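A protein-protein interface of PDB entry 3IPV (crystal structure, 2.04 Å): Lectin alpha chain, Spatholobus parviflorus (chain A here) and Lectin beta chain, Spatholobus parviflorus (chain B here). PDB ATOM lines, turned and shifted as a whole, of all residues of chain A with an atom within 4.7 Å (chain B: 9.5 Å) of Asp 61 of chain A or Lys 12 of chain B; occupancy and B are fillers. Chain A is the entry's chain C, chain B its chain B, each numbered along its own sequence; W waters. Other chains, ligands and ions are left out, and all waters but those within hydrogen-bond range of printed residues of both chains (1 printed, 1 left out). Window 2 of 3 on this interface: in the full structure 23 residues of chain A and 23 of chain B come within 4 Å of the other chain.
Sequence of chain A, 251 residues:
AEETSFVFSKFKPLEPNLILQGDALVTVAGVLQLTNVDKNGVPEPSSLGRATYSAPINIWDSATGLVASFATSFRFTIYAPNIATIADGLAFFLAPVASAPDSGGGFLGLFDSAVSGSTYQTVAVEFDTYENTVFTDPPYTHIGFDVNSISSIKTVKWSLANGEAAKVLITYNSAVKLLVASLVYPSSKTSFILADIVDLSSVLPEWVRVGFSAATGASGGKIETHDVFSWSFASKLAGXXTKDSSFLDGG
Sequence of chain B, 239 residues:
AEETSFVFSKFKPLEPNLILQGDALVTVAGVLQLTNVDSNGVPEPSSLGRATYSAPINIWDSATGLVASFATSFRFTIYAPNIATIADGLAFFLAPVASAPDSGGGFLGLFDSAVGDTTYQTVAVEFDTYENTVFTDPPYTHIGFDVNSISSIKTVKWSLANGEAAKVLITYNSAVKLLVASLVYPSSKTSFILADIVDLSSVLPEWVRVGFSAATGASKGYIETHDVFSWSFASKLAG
The side-chain carboxylate of Glu 2 of chain A is in hydrogen-bond range of the backbone NH of Ser 9 of chain B, at 3.0 Å.
OE2 of Glu 2 of chain A is in hydrogen-bond range of N of Lys 10 of chain B.
The side-chain amino group (NZ) of Lys 12 of chain B lies close to the side-chain amide nitrogen (ND2) of Asn 58 of chain A (2.7 Å).
The side-chain carboxylate of Asp 61 of chain A is in salt-bridge range of the side-chain amino group of Lys 12 of chain B (2.6 Å).
The backbone NH of Glu 2 of chain A lies within hydrogen-bond range of the backbone carbonyl oxygen of Leu 237 of chain A, at 2.9 Å.
The backbone carbonyl oxygen of Trp 60 of chain A sits close to the side-chain amide oxygen of Asn 58 of chain A.
The side-chain amide oxygen of Asn 58 of chain A sits close to the backbone carbonyl oxygen of Glu 206 of chain A (3.1 Å).
The backbone NH (N) of Ala 63 of chain A lies close to the side-chain carboxylate (OD2) of Asp 61 of chain A, at 3.5 Å.
N of Asp 61 of chain A is in hydrogen-bond range of O of Leu 66 of chain A (2.9 Å).
OE1 of Glu 15 of chain B sits at hydrogen-bond distance from N of Lys 12 of chain B (2.7 Å).
Val 7 of chain B touches Glu 2 of chain A (O to CA, 3.4 Å).
OE2 of Glu 2 of chain A touches CA of Phe 8 of chain B, at 3.7 Å.
Leu 237 of chain A touches Lys 12 of chain B (CD2 to NZ, 3.8 Å).
Printed residues of chain B within 4 Å of Glu 2 of chain A: Val 7 (3.4 Å), Phe 8 (3.7 Å), Ser 9 (3.0 Å) and Lys 10 (3.2 Å).
Of the printed residues of chain B, Asn 58 of chain A touches Lys 12 (2.7 Å).
Asp 61 of chain A touches one residue of chain B.
No residue of chain B comes within 4 Å of Ser 62 of chain A.
No residue of chain B comes within 4 Å of Ala 63 of chain A.
No residue of chain B comes within 4 Å of Thr 64 of chain A.
Printed residues of chain A within 4 Å of Val 7 of chain B: Glu 2 (3.4 Å).
Of the printed residues of chain A, Lys 10 of chain B touches Glu 2.
Lys 12 of chain B touches just these residues of chain A: Asn 58 (2.7 Å), Asp 61 (2.6 Å) and Leu 237 (3.8 Å).
The nearest residue of chain B that does not touch Asp 61 of chain A is Lys 10 of chain B (6.2 Å).
Hydrophobic or aromatic side chains of chain A within 4 Å of the printed part of chain B: Leu 237.
Water W1 lies within hydrogen-bond range of the side-chain carboxylate of Glu 2 of chain A, the side-chain amide nitrogen of Asn 58 of chain A and the side-chain carboxylate of Glu 15 of chain B.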
ATOM      1  N   GLU A   2     -27.041  12.829   9.139  1.00  0.00           N
ATOM      2  CA  GLU A   2     -25.771  12.209   9.064  1.00  0.00           C
ATOM      3  C   GLU A   2     -25.614  11.750   7.632  1.00  0.00           C
ATOM      4  O   GLU A   2     -26.426  10.963   7.109  1.00  0.00           O
ATOM      5  CB  GLU A   2     -25.754  10.990   9.986  1.00  0.00           C
ATOM      6  CG  GLU A   2     -26.224  11.304  11.434  1.00  0.00           C
ATOM      7  CD  GLU A   2     -25.207  12.126  12.170  1.00  0.00           C
ATOM      8  OE1 GLU A   2     -24.146  11.573  12.612  1.00  0.00           O
ATOM      9  OE2 GLU A   2     -25.441  13.351  12.252  1.00  0.00           O
ATOM     10  N   ASN A  58     -23.768   5.138   8.293  1.00  0.00           N
ATOM     11  CA  ASN A  58     -24.914   5.022   9.225  1.00  0.00           C
ATOM     12  C   ASN A  58     -26.175   4.868   8.387  1.00  0.00           C
ATOM     13  O   ASN A  58     -26.650   5.806   7.740  1.00  0.00           O
ATOM     14  CB  ASN A  58     -24.961   6.254  10.106  1.00  0.00           C
ATOM     15  CG  ASN A  58     -25.687   6.051  11.424  1.00  0.00           C
ATOM     16  OD1 ASN A  58     -26.262   4.994  11.738  1.00  0.00           O
ATOM     17  ND2 ASN A  58     -25.661   7.094  12.218  1.00  0.00           N
ATOM     18  N   TRP A  60     -29.357   3.304   9.478  1.00  0.00           N
ATOM     19  CA  TRP A  60     -30.592   3.532  10.206  1.00  0.00           C
ATOM     20  C   TRP A  60     -30.212   3.819  11.650  1.00  0.00           C
ATOM     21  O   TRP A  60     -29.047   3.658  12.024  1.00  0.00           O
ATOM     22  CB  TRP A  60     -31.635   2.392  10.068  1.00  0.00           C
ATOM     23  CG  TRP A  60     -31.344   1.029  10.762  1.00  0.00           C
ATOM     24  CD1 TRP A  60     -30.646  -0.015  10.241  1.00  0.00           C
ATOM     25  CD2 TRP A  60     -31.812   0.592  12.051  1.00  0.00           C
ATOM     26  NE1 TRP A  60     -30.616  -1.066  11.141  1.00  0.00           N
ATOM     27  CE2 TRP A  60     -31.307  -0.711  12.263  1.00  0.00           C
ATOM     28  CE3 TRP A  60     -32.603   1.183  13.049  1.00  0.00           C
ATOM     29  CZ2 TRP A  60     -31.595  -1.447  13.392  1.00  0.00           C
ATOM     30  CZ3 TRP A  60     -32.862   0.461  14.195  1.00  0.00           C
ATOM     31  CH2 TRP A  60     -32.334  -0.853  14.366  1.00  0.00           C
ATOM     32  N   ASP A  61     -31.174   4.223  12.483  1.00  0.00           N
ATOM     33  CA  ASP A  61     -30.848   4.743  13.829  1.00  0.00           C
ATOM     34  C   ASP A  61     -31.910   4.254  14.791  1.00  0.00           C
ATOM     35  O   ASP A  61     -33.085   4.458  14.564  1.00  0.00           O
ATOM     36  CB  ASP A  61     -30.803   6.259  13.789  1.00  0.00           C
ATOM     37  CG  ASP A  61     -30.456   6.872  15.111  1.00  0.00           C
ATOM     38  OD1 ASP A  61     -29.288   6.791  15.520  1.00  0.00           O
ATOM     39  OD2 ASP A  61     -31.363   7.454  15.734  1.00  0.00           O
ATOM     40  N   SER A  62     -31.467   3.564  15.843  1.00  0.00           N
ATOM     41  CA  SER A  62     -32.404   2.860  16.714  1.00  0.00           C
ATOM     42  C   SER A  62     -33.100   3.870  17.642  1.00  0.00           C
ATOM     43  O   SER A  62     -34.224   3.679  17.992  1.00  0.00           O
ATOM     44  CB  SER A  62     -31.767   1.672  17.458  1.00  0.00           C
ATOM     45  OG  SER A  62     -30.681   2.079  18.250  1.00  0.00           O
ATOM     46  N   ALA A  63     -32.441   4.984  17.933  1.00  0.00           N
ATOM     47  CA  ALA A  63     -33.036   6.043  18.774  1.00  0.00           C
ATOM     48  C   ALA A  63     -34.249   6.746  18.149  1.00  0.00           C
ATOM     49  O   ALA A  63     -35.267   6.894  18.800  1.00  0.00           O
ATOM     50  CB  ALA A  63     -31.978   7.071  19.144  1.00  0.00           C
ATOM     51  N   THR A  64     -34.114   7.186  16.892  1.00  0.00           N
ATOM     52  CA  THR A  64     -35.190   7.838  16.159  1.00  0.00           C
ATOM     53  C   THR A  64     -36.049   6.831  15.387  1.00  0.00           C
ATOM     54  O   THR A  64     -37.206   7.128  15.025  1.00  0.00           O
ATOM     55  CB  THR A  64     -34.630   8.903  15.146  1.00  0.00           C
ATOM     56  OG1 THR A  64     -33.919   8.243  14.097  1.00  0.00           O
ATOM     57  CG2 THR A  64     -33.700   9.946  15.847  1.00  0.00           C
ATOM     58  N   GLY A  65     -35.492   5.656  15.085  1.00  0.00           N
ATOM     59  CA  GLY A  65     -36.158   4.705  14.166  1.00  0.00           C
ATOM     60  C   GLY A  65     -36.109   5.066  12.669  1.00  0.00           C
ATOM     61  O   GLY A  65     -36.728   4.375  11.844  1.00  0.00           O
ATOM     62  N   LEU A  66     -35.370   6.123  12.311  1.00  0.00           N
ATOM     63  CA  LEU A  66     -35.251   6.534  10.906  1.00  0.00           C
ATOM     64  C   LEU A  66     -34.250   5.655  10.132  1.00  0.00           C
ATOM     65  O   LEU A  66     -33.276   5.119  10.692  1.00  0.00           O
ATOM     66  CB  LEU A  66     -34.858   8.025  10.810  1.00  0.00           C
ATOM     67  CG  LEU A  66     -35.780   8.985  11.623  1.00  0.00           C
ATOM     68  CD1 LEU A  66     -35.649  10.379  11.240  1.00  0.00           C
ATOM     69  CD2 LEU A  66     -37.153   8.568  11.417  1.00  0.00           C
ATOM     70  N   GLU A 206     -27.297  -1.021  12.066  1.00  0.00           N
ATOM     71  CA  GLU A 206     -27.346   0.475  11.907  1.00  0.00           C
ATOM     72  C   GLU A 206     -26.142   1.050  11.109  1.00  0.00           C
ATOM     73  O   GLU A 206     -26.241   2.126  10.514  1.00  0.00           O
ATOM     74  CB  GLU A 206     -27.415   1.184  13.245  1.00  0.00           C
ATOM     75  CG  GLU A 206     -28.685   0.915  14.020  1.00  0.00           C
ATOM     76  CD  GLU A 206     -28.620   1.469  15.408  1.00  0.00           C
ATOM     77  OE1 GLU A 206     -28.719   2.711  15.587  1.00  0.00           O
ATOM     78  OE2 GLU A 206     -28.458   0.639  16.339  1.00  0.00           O
ATOM     79  N   LEU A 237     -29.196  10.219   6.450  1.00  0.00           N
ATOM     80  CA  LEU A 237     -29.939   9.675   7.532  1.00  0.00           C
ATOM     81  C   LEU A 237     -30.427  10.873   8.293  1.00  0.00           C
ATOM     82  O   LEU A 237     -29.615  11.590   8.922  1.00  0.00           O
ATOM     83  CB  LEU A 237     -29.083   8.739   8.406  1.00  0.00           C
ATOM     84  CG  LEU A 237     -29.706   8.196   9.719  1.00  0.00           C
ATOM     85  CD1 LEU A 237     -30.836   7.197   9.368  1.00  0.00           C
ATOM     86  CD2 LEU A 237     -28.684   7.385  10.493  1.00  0.00           C
ATOM     87  N   VAL B   7     -21.141  14.674   6.704  1.00  0.00           N
ATOM     88  CA  VAL B   7     -21.726  15.611   7.644  1.00  0.00           C
ATOM     89  C   VAL B   7     -22.099  14.837   8.932  1.00  0.00           C
ATOM     90  O   VAL B   7     -22.741  13.797   8.878  1.00  0.00           O
ATOM     91  CB  VAL B   7     -22.994  16.269   7.039  1.00  0.00           C
ATOM     92  CG1 VAL B   7     -23.729  17.295   8.039  1.00  0.00           C
ATOM     93  CG2 VAL B   7     -22.672  16.966   5.797  1.00  0.00           C
ATOM     94  N   PHE B   8     -21.750  15.402  10.057  1.00  0.00           N
ATOM     95  CA  PHE B   8     -22.178  14.931  11.346  1.00  0.00           C
ATOM     96  C   PHE B   8     -22.974  16.139  11.852  1.00  0.00           C
ATOM     97  O   PHE B   8     -22.383  17.155  12.267  1.00  0.00           O
ATOM     98  CB  PHE B   8     -20.954  14.760  12.271  1.00  0.00           C
ATOM     99  CG  PHE B   8     -19.963  13.708  11.847  1.00  0.00           C
ATOM    100  CD1 PHE B   8     -20.051  12.413  12.337  1.00  0.00           C
ATOM    101  CD2 PHE B   8     -18.839  14.043  11.060  1.00  0.00           C
ATOM    102  CE1 PHE B   8     -19.077  11.454  11.993  1.00  0.00           C
ATOM    103  CE2 PHE B   8     -17.847  13.092  10.736  1.00  0.00           C
ATOM    104  CZ  PHE B   8     -17.963  11.809  11.180  1.00  0.00           C
ATOM    105  N   SER B   9     -24.286  16.123  11.727  1.00  0.00           N
ATOM    106  CA  SER B   9     -25.064  17.218  12.320  1.00  0.00           C
ATOM    107  C   SER B   9     -25.107  17.091  13.855  1.00  0.00           C
ATOM    108  O   SER B   9     -25.395  18.085  14.576  1.00  0.00           O
ATOM    109  CB  SER B   9     -26.445  17.288  11.761  1.00  0.00           C
ATOM    110  OG  SER B   9     -26.886  18.634  11.870  1.00  0.00           O
ATOM    111  N   LYS B  10     -24.755  15.891  14.313  1.00  0.00           N
ATOM    112  CA  LYS B  10     -24.444  15.565  15.717  1.00  0.00           C
ATOM    113  C   LYS B  10     -23.501  14.408  15.739  1.00  0.00           C
ATOM    114  O   LYS B  10     -23.248  13.820  14.693  1.00  0.00           O
ATOM    115  CB  LYS B  10     -25.704  15.167  16.480  1.00  0.00           C
ATOM    116  CG  LYS B  10     -26.629  14.090  15.822  1.00  0.00           C
ATOM    117  CD  LYS B  10     -27.883  13.824  16.745  1.00  0.00           C
ATOM    118  CE  LYS B  10     -27.863  12.466  17.548  1.00  0.00           C
ATOM    119  NZ  LYS B  10     -26.793  12.075  18.631  1.00  0.00           N
ATOM    120  N   PHE B  11     -22.989  14.037  16.904  1.00  0.00           N
ATOM    121  CA  PHE B  11     -22.178  12.829  17.033  1.00  0.00           C
ATOM    122  C   PHE B  11     -22.968  11.804  17.824  1.00  0.00           C
ATOM    123  O   PHE B  11     -23.948  12.185  18.469  1.00  0.00           O
ATOM    124  CB  PHE B  11     -20.839  13.183  17.732  1.00  0.00           C
ATOM    125  CG  PHE B  11     -20.015  14.207  16.923  1.00  0.00           C
ATOM    126  CD1 PHE B  11     -19.198  13.783  15.909  1.00  0.00           C
ATOM    127  CD2 PHE B  11     -20.161  15.591  17.132  1.00  0.00           C
ATOM    128  CE1 PHE B  11     -18.429  14.696  15.143  1.00  0.00           C
ATOM    129  CE2 PHE B  11     -19.408  16.517  16.358  1.00  0.00           C
ATOM    130  CZ  PHE B  11     -18.586  16.079  15.374  1.00  0.00           C
ATOM    131  N   LYS B  12     -22.568  10.527  17.754  1.00  0.00           N
ATOM    132  CA  LYS B  12     -23.248   9.469  18.496  1.00  0.00           C
ATOM    133  C   LYS B  12     -22.253   8.668  19.285  1.00  0.00           C
ATOM    134  O   LYS B  12     -21.136   8.425  18.826  1.00  0.00           O
ATOM    135  CB  LYS B  12     -24.021   8.521  17.577  1.00  0.00           C
ATOM    136  CG  LYS B  12     -24.558   9.109  16.261  1.00  0.00           C
ATOM    137  CD  LYS B  12     -25.579   8.181  15.625  1.00  0.00           C
ATOM    138  CE  LYS B  12     -26.668   8.972  14.852  1.00  0.00           C
ATOM    139  NZ  LYS B  12     -27.469   7.971  14.045  1.00  0.00           N
ATOM    140  N   PRO B  13     -22.636   8.239  20.482  1.00  0.00           N
ATOM    141  CA  PRO B  13     -21.667   7.470  21.286  1.00  0.00           C
ATOM    142  C   PRO B  13     -21.040   6.253  20.553  1.00  0.00           C
ATOM    143  O   PRO B  13     -19.879   5.918  20.836  1.00  0.00           O
ATOM    144  CB  PRO B  13     -22.472   7.033  22.525  1.00  0.00           C
ATOM    145  CG  PRO B  13     -23.737   7.881  22.530  1.00  0.00           C
ATOM    146  CD  PRO B  13     -23.872   8.583  21.207  1.00  0.00           C
ATOM    147  N   LEU B  14     -21.794   5.580  19.673  1.00  0.00           N
ATOM    148  CA  LEU B  14     -21.204   4.673  18.699  1.00  0.00           C
ATOM    149  C   LEU B  14     -20.984   5.437  17.369  1.00  0.00           C
ATOM    150  O   LEU B  14     -21.952   5.814  16.691  1.00  0.00           O
ATOM    151  CB  LEU B  14     -22.032   3.372  18.475  1.00  0.00           C
ATOM    152  CG  LEU B  14     -21.204   2.127  18.001  1.00  0.00           C
ATOM    153  CD1 LEU B  14     -21.750   1.459  16.765  1.00  0.00           C
ATOM    154  CD2 LEU B  14     -19.743   2.438  17.730  1.00  0.00           C
ATOM    155  N   GLU B  15     -19.729   5.683  17.002  1.00  0.00           N
ATOM    156  CA  GLU B  15     -19.486   6.450  15.792  1.00  0.00           C
ATOM    157  C   GLU B  15     -18.277   5.859  15.086  1.00  0.00           C
ATOM    158  O   GLU B  15     -17.189   6.409  15.188  1.00  0.00           O
ATOM    159  CB  GLU B  15     -19.223   7.891  16.150  1.00  0.00           C
ATOM    160  CG  GLU B  15     -19.187   8.834  15.026  1.00  0.00           C
ATOM    161  CD  GLU B  15     -20.560   9.303  14.669  1.00  0.00           C
ATOM    162  OE1 GLU B  15     -21.161   9.986  15.480  1.00  0.00           O
ATOM    163  OE2 GLU B  15     -21.050   8.967  13.565  1.00  0.00           O
ATOM    164  N   PRO B  16     -18.469   4.735  14.402  1.00  0.00           N
ATOM    165  CA  PRO B  16     -17.311   4.025  13.865  1.00  0.00           C
ATOM    166  C   PRO B  16     -16.586   4.695  12.692  1.00  0.00           C
ATOM    167  O   PRO B  16     -15.492   4.265  12.382  1.00  0.00           O
ATOM    168  CB  PRO B  16     -17.884   2.674  13.402  1.00  0.00           C
ATOM    169  CG  PRO B  16     -19.338   2.832  13.351  1.00  0.00           C
ATOM    170  CD  PRO B  16     -19.690   3.909  14.362  1.00  0.00           C
ATOM    171  N   ASN B  17     -17.163   5.723  12.064  1.00  0.00           N
ATOM    172  CA  ASN B  17     -16.435   6.514  11.027  1.00  0.00           C
ATOM    173  C   ASN B  17     -15.620   7.679  11.601  1.00  0.00           C
ATOM    174  O   ASN B  17     -15.084   8.536  10.887  1.00  0.00           O
ATOM    175  CB  ASN B  17     -17.391   7.014   9.950  1.00  0.00           C
ATOM    176  CG  ASN B  17     -18.599   7.794  10.508  1.00  0.00           C
ATOM    177  OD1 ASN B  17     -18.783   7.972  11.718  1.00  0.00           O
ATOM    178  ND2 ASN B  17     -19.413   8.265   9.603  1.00  0.00           N
ATOM    179  N   LEU B  18     -15.514   7.700  12.922  1.00  0.00           N
ATOM    180  CA  LEU B  18     -14.721   8.700  13.607  1.00  0.00           C
ATOM    181  C   LEU B  18     -13.729   7.927  14.506  1.00  0.00           C
ATOM    182  O   LEU B  18     -14.147   7.168  15.439  1.00  0.00           O
ATOM    183  CB  LEU B  18     -15.657   9.547  14.469  1.00  0.00           C
ATOM    184  CG  LEU B  18     -15.673  11.067  14.582  1.00  0.00           C
ATOM    185  CD1 LEU B  18     -15.903  11.331  16.020  1.00  0.00           C
ATOM    186  CD2 LEU B  18     -14.394  11.798  14.059  1.00  0.00           C
ATOM    187  N   LEU B  20     -11.272   8.053  17.488  1.00  0.00           N
ATOM    188  CA  LEU B  20     -11.090   8.915  18.668  1.00  0.00           C
ATOM    189  C   LEU B  20      -9.756   8.566  19.319  1.00  0.00           C
ATOM    190  O   LEU B  20      -9.472   7.419  19.486  1.00  0.00           O
ATOM    191  CB  LEU B  20     -12.224   8.728  19.665  1.00  0.00           C
ATOM    192  CG  LEU B  20     -13.634   9.084  19.158  1.00  0.00           C
ATOM    193  CD1 LEU B  20     -14.711   8.502  20.106  1.00  0.00           C
ATOM    194  CD2 LEU B  20     -13.784  10.577  18.997  1.00  0.00           C
ATOM    195  N   LEU B  25     -14.193  11.875  23.450  1.00  0.00           N
ATOM    196  CA  LEU B  25     -15.331  11.031  23.523  1.00  0.00           C
ATOM    197  C   LEU B  25     -16.558  11.798  23.094  1.00  0.00           C
ATOM    198  O   LEU B  25     -16.579  13.008  23.098  1.00  0.00           O
ATOM    199  CB  LEU B  25     -15.506  10.527  24.956  1.00  0.00           C
ATOM    200  CG  LEU B  25     -15.765  11.497  26.124  1.00  0.00           C
ATOM    201  CD1 LEU B  25     -17.239  11.582  26.440  1.00  0.00           C
ATOM    202  CD2 LEU B  25     -15.060  11.027  27.366  1.00  0.00           C
ATOM    203  N   VAL B  26     -17.589  11.073  22.745  1.00  0.00           N
ATOM    204  CA  VAL B  26     -18.879  11.621  22.410  1.00  0.00           C
ATOM    205  C   VAL B  26     -19.849  11.347  23.595  1.00  0.00           C
ATOM    206  O   VAL B  26     -19.989  10.209  24.060  1.00  0.00           O
ATOM    207  CB  VAL B  26     -19.386  10.976  21.104  1.00  0.00           C
ATOM    208  CG1 VAL B  26     -20.791  11.394  20.816  1.00  0.00           C
ATOM    209  CG2 VAL B  26     -18.445  11.303  19.869  1.00  0.00           C
ATOM    210  N   THR B  27     -20.498  12.397  24.091  1.00  0.00           N
ATOM    211  CA  THR B  27     -21.462  12.255  25.150  1.00  0.00           C
ATOM    212  C   THR B  27     -22.799  11.691  24.649  1.00  0.00           C
ATOM    213  O   THR B  27     -23.111  11.681  23.418  1.00  0.00           O
ATOM    214  CB  THR B  27     -21.698  13.631  25.863  1.00  0.00           C
ATOM    215  OG1 THR B  27     -22.602  14.423  25.071  1.00  0.00           O
ATOM    216  CG2 THR B  27     -20.349  14.390  26.068  1.00  0.00           C
ATOM    217  N   VAL B  28     -23.613  11.259  25.616  1.00  0.00           N
ATOM    218  CA  VAL B  28     -24.933  10.741  25.304  1.00  0.00           C
ATOM    219  C   VAL B  28     -25.741  11.819  24.569  1.00  0.00           C
ATOM    220  O   VAL B  28     -26.624  11.483  23.836  1.00  0.00           O
ATOM    221  CB  VAL B  28     -25.727  10.403  26.602  1.00  0.00           C
ATOM    222  CG1 VAL B  28     -27.010   9.831  26.248  1.00  0.00           C
ATOM    223  CG2 VAL B  28     -25.030   9.392  27.459  1.00  0.00           C
ATOM    224  N   ALA B  29     -25.459  13.104  24.822  1.00  0.00           N
ATOM    225  CA  ALA B  29     -26.181  14.280  24.242  1.00  0.00           C
ATOM    226  C   ALA B  29     -25.754  14.574  22.780  1.00  0.00           C
ATOM    227  O   ALA B  29     -26.305  15.467  22.135  1.00  0.00           O
ATOM    228  CB  ALA B  29     -25.861  15.550  25.090  1.00  0.00           C
ATOM    229  N   GLY B  30     -24.751  13.859  22.268  1.00  0.00           N
ATOM    230  CA  GLY B  30     -24.273  14.078  20.887  1.00  0.00           C
ATOM    231  C   GLY B  30     -23.127  15.053  20.702  1.00  0.00           C
ATOM    232  O   GLY B  30     -22.851  15.463  19.571  1.00  0.00           O
ATOM    233  N   VAL B  31     -22.485  15.453  21.801  1.00  0.00           N
ATOM    234  CA  VAL B  31     -21.366  16.371  21.723  1.00  0.00           C
ATOM    235  C   VAL B  31     -20.024  15.616  21.785  1.00  0.00           C
ATOM    236  O   VAL B  31     -19.862  14.705  22.544  1.00  0.00           O
ATOM    237  CB  VAL B  31     -21.447  17.605  22.745  1.00  0.00           C
ATOM    238  CG1 VAL B  31     -22.798  17.724  23.420  1.00  0.00           C
ATOM    239  CG2 VAL B  31     -20.303  17.653  23.740  1.00  0.00           C
ATOM    240  N   LEU B  32     -19.097  16.017  20.922  1.00  0.00           N
ATOM    241  CA  LEU B  32     -17.759  15.479  20.848  1.00  0.00           C
ATOM    242  C   LEU B  32     -16.920  16.332  21.844  1.00  0.00           C
ATOM    243  O   LEU B  32     -16.648  17.485  21.556  1.00  0.00           O
ATOM    244  CB  LEU B  32     -17.241  15.551  19.376  1.00  0.00           C
ATOM    245  CG  LEU B  32     -15.734  15.336  19.135  1.00  0.00           C
ATOM    246  CD1 LEU B  32     -15.349  13.903  19.535  1.00  0.00           C
ATOM    247  CD2 LEU B  32     -15.382  15.582  17.668  1.00  0.00           C
ATOM    248  N   VAL B 228     -17.085  20.005  20.300  1.00  0.00           N
ATOM    249  CA  VAL B 228     -17.526  20.162  18.918  1.00  0.00           C
ATOM    250  C   VAL B 228     -18.996  19.642  18.881  1.00  0.00           C
ATOM    251  O   VAL B 228     -19.275  18.569  19.372  1.00  0.00           O
ATOM    252  CB  VAL B 228     -16.619  19.438  17.898  1.00  0.00           C
ATOM    253  CG1 VAL B 228     -17.133  19.712  16.430  1.00  0.00           C
ATOM    254  CG2 VAL B 228     -15.163  19.907  18.047  1.00  0.00           C
ATOM    255  N   PHE B 229     -19.903  20.432  18.304  1.00  0.00           N
ATOM    256  CA  PHE B 229     -21.313  20.095  18.212  1.00  0.00           C
ATOM    257  C   PHE B 229     -21.678  19.499  16.892  1.00  0.00           C
ATOM    258  O   PHE B 229     -22.614  18.710  16.850  1.00  0.00           O
ATOM    259  CB  PHE B 229     -22.146  21.338  18.331  1.00  0.00           C
ATOM    260  CG  PHE B 229     -21.851  22.074  19.537  1.00  0.00           C
ATOM    261  CD1 PHE B 229     -21.893  21.432  20.731  1.00  0.00           C
ATOM    262  CD2 PHE B 229     -21.442  23.388  19.484  1.00  0.00           C
ATOM    263  CE1 PHE B 229     -21.557  22.054  21.831  1.00  0.00           C
ATOM    264  CE2 PHE B 229     -21.165  23.982  20.576  1.00  0.00           C
ATOM    265  CZ  PHE B 229     -21.207  23.310  21.763  1.00  0.00           C
HETATM  266  O   HOH W   1     -23.621   9.118  12.157  1.00  0.00           O
